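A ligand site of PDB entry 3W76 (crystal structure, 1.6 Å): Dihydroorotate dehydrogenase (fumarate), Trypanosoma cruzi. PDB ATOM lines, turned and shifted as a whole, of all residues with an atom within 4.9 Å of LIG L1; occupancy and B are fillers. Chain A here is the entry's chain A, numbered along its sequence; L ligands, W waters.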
ATOM      1  N   ALA A  19     -12.059  -5.107  18.359  1.00  0.00           N
ATOM      2  CA  ALA A  19     -12.155  -6.477  17.911  1.00  0.00           C
ATOM      3  C   ALA A  19     -13.628  -6.853  17.702  1.00  0.00           C
ATOM      4  O   ALA A  19     -14.496  -6.489  18.516  1.00  0.00           O
ATOM      5  CB  ALA A  19     -11.487  -7.425  18.876  1.00  0.00           C
ATOM      6  N   ALA A  20     -13.904  -7.592  16.630  1.00  0.00           N
ATOM      7  CA  ALA A  20     -15.277  -7.998  16.430  1.00  0.00           C
ATOM      8  C   ALA A  20     -15.843  -8.678  17.637  1.00  0.00           C
ATOM      9  O   ALA A  20     -15.153  -9.478  18.317  1.00  0.00           O
ATOM     10  CB  ALA A  20     -15.422  -8.850  15.191  1.00  0.00           C
ATOM     11  N   GLY A  21     -17.085  -8.380  17.985  1.00  0.00           N
ATOM     12  CA  GLY A  21     -17.747  -8.939  19.137  1.00  0.00           C
ATOM     13  C   GLY A  21     -17.731  -8.084  20.396  1.00  0.00           C
ATOM     14  O   GLY A  21     -18.625  -8.226  21.255  1.00  0.00           O
ATOM     15  N   VAL A  22     -16.719  -7.165  20.494  1.00  0.00           N
ATOM     16  CA  VAL A  22     -16.616  -6.305  21.662  1.00  0.00           C
ATOM     17  C   VAL A  22     -17.136  -4.915  21.361  1.00  0.00           C
ATOM     18  O   VAL A  22     -16.717  -4.273  20.402  1.00  0.00           O
ATOM     19  CB  VAL A  22     -15.154  -6.246  22.165  1.00  0.00           C
ATOM     20  CG1 VAL A  22     -15.046  -5.326  23.376  1.00  0.00           C
ATOM     21  CG2 VAL A  22     -14.679  -7.633  22.502  1.00  0.00           C
ATOM     22  N   LYS A  44     -20.436  -6.650  15.329  1.00  0.00           N
ATOM     23  CA  LYS A  44     -20.510  -8.007  15.841  1.00  0.00           C
ATOM     24  C   LYS A  44     -20.723  -8.931  14.673  1.00  0.00           C
ATOM     25  O   LYS A  44     -21.516  -8.666  13.784  1.00  0.00           O
ATOM     26  CB  LYS A  44     -21.733  -8.111  16.784  1.00  0.00           C
ATOM     27  CG  LYS A  44     -22.059  -9.533  17.244  1.00  0.00           C
ATOM     28  CD  LYS A  44     -21.023 -10.223  18.134  1.00  0.00           C
ATOM     29  CE  LYS A  44     -21.261 -11.718  18.331  1.00  0.00           C
ATOM     30  NZ  LYS A  44     -20.186 -12.333  19.155  1.00  0.00           N
ATOM     31  N   SER A  45     -20.094 -10.113  14.685  1.00  0.00           N
ATOM     32  CA  SER A  45     -20.284 -11.043  13.593  1.00  0.00           C
ATOM     33  C   SER A  45     -21.765 -11.428  13.586  1.00  0.00           C
ATOM     34  O   SER A  45     -22.359 -11.749  14.604  1.00  0.00           O
ATOM     35  CB  SER A  45     -19.514 -12.334  13.791  1.00  0.00           C
ATOM     36  OG  SER A  45     -18.118 -12.113  13.663  1.00  0.00           O
ATOM     37  N   TYR A  59     -19.168 -14.888  29.384  1.00  0.00           N
ATOM     38  CA  TYR A  59     -17.927 -14.135  29.330  1.00  0.00           C
ATOM     39  C   TYR A  59     -17.452 -13.893  30.739  1.00  0.00           C
ATOM     40  O   TYR A  59     -18.197 -13.470  31.630  1.00  0.00           O
ATOM     41  CB  TYR A  59     -18.103 -12.796  28.680  1.00  0.00           C
ATOM     42  CG  TYR A  59     -16.889 -11.868  28.757  1.00  0.00           C
ATOM     43  CD1 TYR A  59     -15.874 -11.974  27.836  1.00  0.00           C
ATOM     44  CD2 TYR A  59     -16.770 -10.919  29.776  1.00  0.00           C
ATOM     45  CE1 TYR A  59     -14.794 -11.150  27.860  1.00  0.00           C
ATOM     46  CE2 TYR A  59     -15.649 -10.094  29.801  1.00  0.00           C
ATOM     47  CZ  TYR A  59     -14.657 -10.233  28.885  1.00  0.00           C
ATOM     48  OH  TYR A  59     -13.577  -9.402  28.968  1.00  0.00           O
ATOM     49  N   SER A  66      -9.346 -13.205  29.202  1.00  0.00           N
ATOM     50  CA  SER A  66     -10.740 -13.514  29.230  1.00  0.00           C
ATOM     51  C   SER A  66     -11.031 -14.859  28.583  1.00  0.00           C
ATOM     52  O   SER A  66     -10.261 -15.400  27.801  1.00  0.00           O
ATOM     53  CB  SER A  66     -11.578 -12.464  28.515  1.00  0.00           C
ATOM     54  OG  SER A  66     -11.318 -12.485  27.114  1.00  0.00           O
ATOM     55  N   ASN A  68     -14.614 -16.744  26.707  1.00  0.00           N
ATOM     56  CA  ASN A  68     -16.012 -16.516  26.251  1.00  0.00           C
ATOM     57  C   ASN A  68     -16.508 -17.714  25.483  1.00  0.00           C
ATOM     58  O   ASN A  68     -15.826 -18.292  24.637  1.00  0.00           O
ATOM     59  CB  ASN A  68     -16.139 -15.237  25.455  1.00  0.00           C
ATOM     60  CG  ASN A  68     -15.886 -15.369  23.973  1.00  0.00           C
ATOM     61  OD1 ASN A  68     -16.728 -15.793  23.185  1.00  0.00           O
ATOM     62  ND2 ASN A  68     -14.700 -15.084  23.583  1.00  0.00           N
ATOM     63  N   MET A  70     -19.848 -16.958  23.795  1.00  0.00           N
ATOM     64  CA  MET A  70     -20.999 -16.133  23.629  1.00  0.00           C
ATOM     65  C   MET A  70     -22.082 -16.846  22.842  1.00  0.00           C
ATOM     66  O   MET A  70     -23.275 -16.633  23.177  1.00  0.00           O
ATOM     67  CB  MET A  70     -20.653 -14.823  23.005  1.00  0.00           C
ATOM     68  CG  MET A  70     -19.609 -13.939  23.621  1.00  0.00           C
ATOM     69  SD  MET A  70     -19.932 -13.521  25.315  1.00  0.00           S
ATOM     70  CE  MET A  70     -21.156 -12.343  25.118  1.00  0.00           C
ATOM     71  N   LEU A  72     -22.467 -16.462  19.329  1.00  0.00           N
ATOM     72  CA  LEU A  72     -22.882 -15.578  18.279  1.00  0.00           C
ATOM     73  C   LEU A  72     -24.197 -14.863  18.548  1.00  0.00           C
ATOM     74  O   LEU A  72     -25.034 -14.738  17.624  1.00  0.00           O
ATOM     75  CB  LEU A  72     -22.854 -16.370  16.987  1.00  0.00           C
ATOM     76  CG  LEU A  72     -22.640 -15.904  15.614  1.00  0.00           C
ATOM     77  CD1 LEU A  72     -21.528 -14.873  15.497  1.00  0.00           C
ATOM     78  CD2 LEU A  72     -22.314 -17.225  14.848  1.00  0.00           C
ATOM     79  N   SER A  98     -18.694  -7.558  10.139  1.00  0.00           N
ATOM     80  CA  SER A  98     -18.247  -8.958  10.261  1.00  0.00           C
ATOM     81  C   SER A  98     -19.423  -9.848  10.018  1.00  0.00           C
ATOM     82  O   SER A  98     -20.534  -9.690  10.579  1.00  0.00           O
ATOM     83  CB  SER A  98     -17.685  -9.193  11.638  1.00  0.00           C
ATOM     84  OG  SER A  98     -17.365 -10.552  11.763  1.00  0.00           O
ATOM     85  N   GLU A 126     -15.397  -8.036   6.801  1.00  0.00           N
ATOM     86  CA  GLU A 126     -14.534  -8.998   7.481  1.00  0.00           C
ATOM     87  C   GLU A 126     -15.294 -10.296   7.643  1.00  0.00           C
ATOM     88  O   GLU A 126     -16.285 -10.370   8.360  1.00  0.00           O
ATOM     89  CB  GLU A 126     -13.964  -8.402   8.828  1.00  0.00           C
ATOM     90  CG  GLU A 126     -12.971  -9.375   9.560  1.00  0.00           C
ATOM     91  CD  GLU A 126     -12.485  -8.803  10.908  1.00  0.00           C
ATOM     92  OE1 GLU A 126     -13.187  -8.975  11.957  1.00  0.00           O
ATOM     93  OE2 GLU A 126     -11.406  -8.137  10.988  1.00  0.00           O
ATOM     94  N   ASN A 128     -15.722 -13.851   9.031  1.00  0.00           N
ATOM     95  CA  ASN A 128     -15.275 -14.656  10.152  1.00  0.00           C
ATOM     96  C   ASN A 128     -15.346 -16.129   9.865  1.00  0.00           C
ATOM     97  O   ASN A 128     -16.445 -16.634   9.732  1.00  0.00           O
ATOM     98  CB  ASN A 128     -16.113 -14.291  11.381  1.00  0.00           C
ATOM     99  CG  ASN A 128     -15.720 -15.047  12.634  1.00  0.00           C
ATOM    100  OD1 ASN A 128     -14.790 -15.830  12.673  1.00  0.00           O
ATOM    101  ND2 ASN A 128     -16.473 -14.862  13.657  1.00  0.00           N
ATOM    102  N   LYS A 165     -11.173 -12.999   8.996  1.00  0.00           N
ATOM    103  CA  LYS A 165     -10.781 -13.209  10.438  1.00  0.00           C
ATOM    104  C   LYS A 165     -10.396 -14.701  10.621  1.00  0.00           C
ATOM    105  O   LYS A 165     -11.219 -15.590  10.412  1.00  0.00           O
ATOM    106  CB  LYS A 165     -11.913 -12.781  11.338  1.00  0.00           C
ATOM    107  CG  LYS A 165     -11.659 -12.965  12.848  1.00  0.00           C
ATOM    108  CD  LYS A 165     -10.762 -11.910  13.309  1.00  0.00           C
ATOM    109  CE  LYS A 165     -10.668 -11.897  14.815  1.00  0.00           C
ATOM    110  NZ  LYS A 165     -11.854 -11.329  15.469  1.00  0.00           N
ATOM    111  N   VAL A 194      -5.512 -12.488  15.457  1.00  0.00           N
ATOM    112  CA  VAL A 194      -6.255 -13.722  15.488  1.00  0.00           C
ATOM    113  C   VAL A 194      -7.555 -13.585  16.218  1.00  0.00           C
ATOM    114  O   VAL A 194      -7.714 -12.651  17.053  1.00  0.00           O
ATOM    115  CB  VAL A 194      -5.407 -14.813  16.181  1.00  0.00           C
ATOM    116  CG1 VAL A 194      -4.215 -15.234  15.324  1.00  0.00           C
ATOM    117  CG2 VAL A 194      -5.021 -14.416  17.613  1.00  0.00           C
ATOM    118  N   ASN A 195      -8.471 -14.529  15.921  1.00  0.00           N
ATOM    119  CA  ASN A 195      -9.572 -14.818  16.818  1.00  0.00           C
ATOM    120  C   ASN A 195      -9.073 -15.396  18.138  1.00  0.00           C
ATOM    121  O   ASN A 195      -7.856 -15.666  18.341  1.00  0.00           O
ATOM    122  CB  ASN A 195     -10.559 -15.763  16.104  1.00  0.00           C
ATOM    123  CG  ASN A 195     -11.993 -15.475  16.473  1.00  0.00           C
ATOM    124  OD1 ASN A 195     -12.349 -15.340  17.645  1.00  0.00           O
ATOM    125  ND2 ASN A 195     -12.878 -15.439  15.448  1.00  0.00           N
ATOM    126  N   SER A 196      -9.968 -15.601  19.097  1.00  0.00           N
ATOM    127  CA  SER A 196      -9.649 -16.137  20.407  1.00  0.00           C
ATOM    128  C   SER A 196      -9.001 -17.525  20.262  1.00  0.00           C
ATOM    129  O   SER A 196      -9.201 -18.256  19.266  1.00  0.00           O
ATOM    130  CB  SER A 196     -10.922 -16.106  21.313  1.00  0.00           C
ATOM    131  OG  SER A 196     -11.918 -16.847  20.754  1.00  0.00           O
ATOM    132  N   GLY A 222      -8.866 -14.807  25.285  1.00  0.00           N
ATOM    133  CA  GLY A 222      -8.302 -13.560  24.792  1.00  0.00           C
ATOM    134  C   GLY A 222      -7.421 -12.968  25.867  1.00  0.00           C
ATOM    135  O   GLY A 222      -7.403 -13.420  27.026  1.00  0.00           O
ATOM    136  N   GLY A 223      -6.781 -11.848  25.488  1.00  0.00           N
ATOM    137  CA  GLY A 223      -6.012 -11.112  26.456  1.00  0.00           C
ATOM    138  C   GLY A 223      -4.556 -11.471  26.573  1.00  0.00           C
ATOM    139  O   GLY A 223      -3.943 -11.951  25.607  1.00  0.00           O
ATOM    140  N   ILE A 226      -2.627 -14.572  25.192  1.00  0.00           N
ATOM    141  CA  ILE A 226      -2.508 -14.919  23.807  1.00  0.00           C
ATOM    142  C   ILE A 226      -1.637 -14.004  22.958  1.00  0.00           C
ATOM    143  O   ILE A 226      -1.495 -14.216  21.785  1.00  0.00           O
ATOM    144  CB  ILE A 226      -3.916 -15.028  23.123  1.00  0.00           C
ATOM    145  CG1 ILE A 226      -4.591 -13.681  22.716  1.00  0.00           C
ATOM    146  CG2 ILE A 226      -4.890 -15.854  23.957  1.00  0.00           C
ATOM    147  CD1 ILE A 226      -5.705 -13.834  21.691  1.00  0.00           C
ATOM    148  N   CYS A 249      -4.698  -8.762  16.031  1.00  0.00           N
ATOM    149  CA  CYS A 249      -5.646  -8.838  17.125  1.00  0.00           C
ATOM    150  C   CYS A 249      -5.153  -9.837  18.124  1.00  0.00           C
ATOM    151  O   CYS A 249      -4.827 -10.961  17.748  1.00  0.00           O
ATOM    152  CB  CYS A 249      -6.986  -9.321  16.577  1.00  0.00           C
ATOM    153  SG  CYS A 249      -8.357  -9.129  17.810  1.00  0.00           S
ATOM    154  N   GLY A 250      -5.097  -9.463  19.378  1.00  0.00           N
ATOM    155  CA  GLY A 250      -4.802 -10.409  20.429  1.00  0.00           C
ATOM    156  C   GLY A 250      -3.861  -9.818  21.436  1.00  0.00           C
ATOM    157  O   GLY A 250      -2.717  -9.487  21.124  1.00  0.00           O
ATOM    158  N   GLY A 251      -4.308  -9.668  22.661  1.00  0.00           N
ATOM    159  CA  GLY A 251      -3.452  -9.283  23.745  1.00  0.00           C
ATOM    160  C   GLY A 251      -2.979  -7.875  23.795  1.00  0.00           C
ATOM    161  O   GLY A 251      -2.019  -7.553  24.515  1.00  0.00           O
ATOM    162  N   VAL A 252      -3.705  -6.954  23.109  1.00  0.00           N
ATOM    163  CA  VAL A 252      -3.272  -5.580  23.132  1.00  0.00           C
ATOM    164  C   VAL A 252      -3.901  -4.890  24.392  1.00  0.00           C
ATOM    165  O   VAL A 252      -5.149  -4.758  24.470  1.00  0.00           O
ATOM    166  CB  VAL A 252      -3.678  -4.837  21.880  1.00  0.00           C
ATOM    167  CG1 VAL A 252      -3.360  -3.340  22.032  1.00  0.00           C
ATOM    168  CG2 VAL A 252      -2.991  -5.479  20.683  1.00  0.00           C
ATOM    169  N   GLN A 270      -6.416  -4.374  16.494  1.00  0.00           N
ATOM    170  CA  GLN A 270      -7.737  -4.549  17.029  1.00  0.00           C
ATOM    171  C   GLN A 270      -7.590  -4.871  18.556  1.00  0.00           C
ATOM    172  O   GLN A 270      -6.624  -5.493  18.990  1.00  0.00           O
ATOM    173  CB  GLN A 270      -8.493  -5.672  16.428  1.00  0.00           C
ATOM    174  CG  GLN A 270      -8.528  -5.590  14.898  1.00  0.00           C
ATOM    175  CD  GLN A 270      -9.488  -6.537  14.282  1.00  0.00           C
ATOM    176  OE1 GLN A 270      -9.821  -7.589  14.848  1.00  0.00           O
ATOM    177  NE2 GLN A 270      -9.997  -6.165  13.120  1.00  0.00           N
ATOM    178  N   VAL A 271      -8.578  -4.394  19.304  1.00  0.00           N
ATOM    179  CA  VAL A 271      -8.536  -4.506  20.777  1.00  0.00           C
ATOM    180  C   VAL A 271      -9.877  -5.136  21.292  1.00  0.00           C
ATOM    181  O   VAL A 271     -10.959  -4.557  21.050  1.00  0.00           O
ATOM    182  CB  VAL A 271      -8.380  -3.074  21.407  1.00  0.00           C
ATOM    183  CG1 VAL A 271      -8.230  -3.193  22.921  1.00  0.00           C
ATOM    184  CG2 VAL A 271      -7.193  -2.355  20.763  1.00  0.00           C
ATOM    185  N   GLY A 272      -9.747  -6.321  21.913  1.00  0.00           N
ATOM    186  CA  GLY A 272     -10.898  -7.067  22.375  1.00  0.00           C
ATOM    187  C   GLY A 272     -11.031  -6.984  23.874  1.00  0.00           C
ATOM    188  O   GLY A 272     -11.680  -6.079  24.374  1.00  0.00           O
ATOM    189  N   THR A 273     -10.489  -7.985  24.555  1.00  0.00           N
ATOM    190  CA  THR A 273     -10.567  -8.072  26.028  1.00  0.00           C
ATOM    191  C   THR A 273     -10.267  -6.768  26.703  1.00  0.00           C
ATOM    192  O   THR A 273     -11.007  -6.382  27.595  1.00  0.00           O
ATOM    193  CB  THR A 273      -9.593  -9.193  26.517  1.00  0.00           C
ATOM    194  OG1 THR A 273      -9.955 -10.439  25.917  1.00  0.00           O
ATOM    195  CG2 THR A 273      -9.658  -9.291  28.008  1.00  0.00           C
ATOM    196  N   ALA A 274      -9.120  -6.148  26.376  1.00  0.00           N
ATOM    197  CA  ALA A 274      -8.792  -4.909  27.081  1.00  0.00           C
ATOM    198  C   ALA A 274      -9.849  -3.801  26.957  1.00  0.00           C
ATOM    199  O   ALA A 274     -10.035  -3.031  27.873  1.00  0.00           O
ATOM    200  CB  ALA A 274      -7.423  -4.432  26.663  1.00  0.00           C
HETATM  201  N1  LIG L   1     -14.402 -12.498  17.047  1.00  0.00           N
HETATM  202  C1  LIG L   1     -15.109 -12.437  15.906  1.00  0.00           C
HETATM  203  O1  LIG L   1     -14.489 -12.378  14.823  1.00  0.00           O
HETATM  204  N2  LIG L   1     -16.448 -12.259  15.896  1.00  0.00           N
HETATM  205  C2  LIG L   1     -17.172 -12.175  16.987  1.00  0.00           C
HETATM  206  O2  LIG L   1     -18.416 -11.944  17.014  1.00  0.00           O
HETATM  207  C3  LIG L   1     -16.471 -12.215  18.255  1.00  0.00           C
HETATM  208  N3  LIG L   1     -17.127 -12.107  19.426  1.00  0.00           N
HETATM  209  C4  LIG L   1     -16.392 -11.915  20.536  1.00  0.00           C
HETATM  210  C5  LIG L   1     -17.030 -11.722  21.753  1.00  0.00           C
HETATM  211  C6  LIG L   1     -16.301 -11.527  22.950  1.00  0.00           C
HETATM  212  C7  LIG L   1     -17.026 -11.212  24.278  1.00  0.00           C
HETATM  213  C8  LIG L   1     -14.887 -11.663  22.948  1.00  0.00           C
HETATM  214  C9  LIG L   1     -14.064 -11.548  24.156  1.00  0.00           C
HETATM  215  C10 LIG L   1     -14.270 -11.933  21.730  1.00  0.00           C
HETATM  216  C11 LIG L   1     -14.965 -12.073  20.571  1.00  0.00           C
HETATM  217  N4  LIG L   1     -14.312 -12.344  19.384  1.00  0.00           N
HETATM  218  C12 LIG L   1     -15.024 -12.326  18.186  1.00  0.00           C
HETATM  219  C13 LIG L   1     -12.870 -12.498  19.259  1.00  0.00           C
HETATM  220  C14 LIG L   1     -12.210 -11.132  19.303  1.00  0.00           C
HETATM  221  O3  LIG L   1     -12.538 -10.391  18.147  1.00  0.00           O
HETATM  222  C15 LIG L   1     -10.682 -11.258  19.364  1.00  0.00           C
HETATM  223  O4  LIG L   1     -10.280 -11.957  18.159  1.00  0.00           O
HETATM  224  C16 LIG L   1     -10.142 -12.032  20.592  1.00  0.00           C
HETATM  225  O5  LIG L   1     -10.894 -11.668  21.786  1.00  0.00           O
HETATM  226  C17 LIG L   1      -8.663 -11.780  20.803  1.00  0.00           C
HETATM  227  O6  LIG L   1      -8.330 -10.425  21.033  1.00  0.00           O
HETATM  228  P1  LIG L   1      -8.059  -9.906  22.543  1.00  0.00           P
HETATM  229  O7  LIG L   1      -7.875  -8.448  22.363  1.00  0.00           O
HETATM  230  O8  LIG L   1      -6.871 -10.657  23.054  1.00  0.00           O
HETATM  231  O9  LIG L   1      -9.325 -10.174  23.353  1.00  0.00           O
HETATM  232  O1  LG2 L   2     -18.871 -16.794  20.947  1.00  0.00           O
HETATM  233  C1  LG2 L   2     -18.862 -15.895  20.031  1.00  0.00           C
HETATM  234  O2  LG2 L   2     -19.872 -15.216  19.655  1.00  0.00           O
HETATM  235  C2  LG2 L   2     -17.554 -15.739  19.372  1.00  0.00           C
HETATM  236  N1  LG2 L   2     -16.492 -15.631  20.304  1.00  0.00           N
HETATM  237  C3  LG2 L   2     -15.198 -15.551  19.860  1.00  0.00           C
HETATM  238  O3  LG2 L   2     -14.234 -15.431  20.693  1.00  0.00           O
HETATM  239  N2  LG2 L   2     -14.967 -15.490  18.533  1.00  0.00           N
HETATM  240  C4  LG2 L   2     -15.985 -15.567  17.591  1.00  0.00           C
HETATM  241  O4  LG2 L   2     -15.642 -15.563  16.419  1.00  0.00           O
HETATM  242  C5  LG2 L   2     -17.307 -15.692  18.026  1.00  0.00           C
HETATM  243  C6  LG2 L   2     -18.447 -15.837  17.078  1.00  0.00           C
HETATM  244  C7  LG2 L   2     -18.299 -17.117  16.317  1.00  0.00           C
HETATM  245  C8  LG2 L   2     -18.248 -18.214  17.187  1.00  0.00           C
HETATM  246  C9  LG2 L   2     -19.151 -18.507  18.227  1.00  0.00           C
HETATM  247  C10 LG2 L   2     -17.179 -19.104  17.168  1.00  0.00           C
HETATM  248  C11 LG2 L   2     -17.022 -20.174  18.041  1.00  0.00           C
HETATM  249  C12 LG2 L   2     -17.929 -20.501  19.019  1.00  0.00           C
HETATM  250  C13 LG2 L   2     -19.016 -19.603  19.114  1.00  0.00           C
HETATM  251  O5  LG2 L   2     -20.003 -19.658  20.022  1.00  0.00           O
HETATM  252  C14 LG2 L   2     -19.818 -20.409  21.248  1.00  0.00           C
HETATM  253  O   HOH W   1      -7.123  -6.936  24.518  1.00  0.00           O
HETATM  254  O   HOH W   2     -14.869 -11.080  12.283  1.00  0.00           O
HETATM  255  O   HOH W   3     -12.561 -14.403  25.500  1.00  0.00           O
HETATM  256  O   HOH W   4      -5.851  -7.265  21.003  1.00  0.00           O
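An oxygen (O9) of LIG L1 is in hydrogen-bond range of the backbone NH (N) of Thr 273 (2.8 Å).
An oxygen (O9) of LIG L1 lies within hydrogen-bond range of the side-chain hydroxyl (OG1) of Thr 273.
O8 of LIG L1 is in hydrogen-bond range of N of Gly 223, 2.7 Å away.
N of Gly 251 is in hydrogen-bond range of O8 of LIG L1.
N of Ala 20 sits at hydrogen-bond distance from O3 of LIG L1 (3.5 Å).
The backbone carbonyl oxygen (O) of Ala 20 is in hydrogen-bond range of an oxygen (O3) of LIG L1 (2.8 Å).
An oxygen (O2) of LIG L1 sits at hydrogen-bond distance from the backbone NH (N) of Ser 45 (3.4 Å).
A nitrogen (N2) of LIG L1 sits at hydrogen-bond distance from the side-chain hydroxyl of Ser 45 (2.8 Å).
NZ of Lys 44 lies within hydrogen-bond range of O2 of LIG L1 (2.8 Å).
N of Gly 272 sits at hydrogen-bond distance from O7 of LIG L1, at 2.9 Å.
The backbone carbonyl oxygen (O) of Val 194 sits at hydrogen-bond distance from an oxygen (O4) of LIG L1, 2.9 Å away.
The side-chain amino group (NZ) of Lys 165 lies within hydrogen-bond range of an oxygen (O1) of LIG L1, at 2.9 Å.
The side-chain amide nitrogen (ND2) of Asn 128 sits at hydrogen-bond distance from an oxygen (O1) of LIG L1.
O4 of LIG L1 is in hydrogen-bond range of SG of Cys 249 (3.4 Å).
The side-chain amino group (NZ) of Lys 44 lies within salt-bridge range of an oxygen (O2) of LG2 L2, at 2.9 Å.
OD1 of Asn 195 is in hydrogen-bond range of N2 of LG2 L2, at 2.8 Å.
An oxygen (O4) of LG2 L2 is in hydrogen-bond range of the side-chain amide nitrogen (ND2) of Asn 128 (3.0 Å).
The side-chain amide oxygen of Asn 68 sits at hydrogen-bond distance from a nitrogen (N1) of LG2 L2 (2.9 Å).
The side-chain hydroxyl (OG) of Ser 196 lies within hydrogen-bond range of an oxygen (O3) of LG2 L2 (2.7 Å).
O1 of LG2 L2 sits at hydrogen-bond distance from N of Met 70.
The backbone NH (N) of Leu 72 lies within hydrogen-bond range of an oxygen (O2) of LG2 L2.
A nitrogen (N2) of LG2 L2 sits close to a nitrogen (N1) of LIG L1 (3.4 Å).
The side-chain hydroxyl of Thr 273 is in hydrogen-bond range of the backbone NH of Gly 223 (3.5 Å).
OG of Ser 66 is in hydrogen-bond range of OG1 of Thr 273 (2.7 Å).
The side-chain hydroxyl of Ser 45 lies within hydrogen-bond range of the side-chain amide nitrogen of Asn 128, at 3.2 Å.
The backbone NH of Val 194 lies within hydrogen-bond range of the backbone carbonyl oxygen of Cys 249, 2.8 Å away.
ND2 of Asn 195 is in hydrogen-bond range of OD1 of Asn 128, at 3.4 Å.
The side-chain amide oxygen (OD1) of Asn 195 sits at hydrogen-bond distance from the side-chain hydroxyl (OG) of Ser 196, 3.5 Å away.
SG of Cys 249 is in hydrogen-bond range of OE1 of Gln 270, 3.6 Å away.
O of Gly 222 lies within hydrogen-bond range of N of Ser 66, at 2.9 Å.
Merely in contact with LIG L1: Ala 19, Asn 195, Gly 21, Gly 250, Asn 68, Ile 226, Gly 222, Ser 196, Tyr 59 and Met 70.
Hydrophobic or aromatic side chains within 4 Å of LIG L1: Ala 19, Ala 20, Tyr 59, Met 70 and Ile 226.
The nearest printed residue that does not touch LIG L1 is Val 271 (4.02 Å).
Water W1 lies within hydrogen-bond range of an oxygen (O7) of LIG L1, the backbone NH (N) of Ala 274 and the backbone carbonyl oxygen (O) of Val 252.
Water W2 lies within hydrogen-bond range of OG of Ser 98, OE1 of Glu 126 and O1 of LIG L1.
Water W3 bridges the side-chain hydroxyl of Ser 66 (2.8 Å) and the side-chain amide nitrogen of Asn 68 (3.0 Å).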
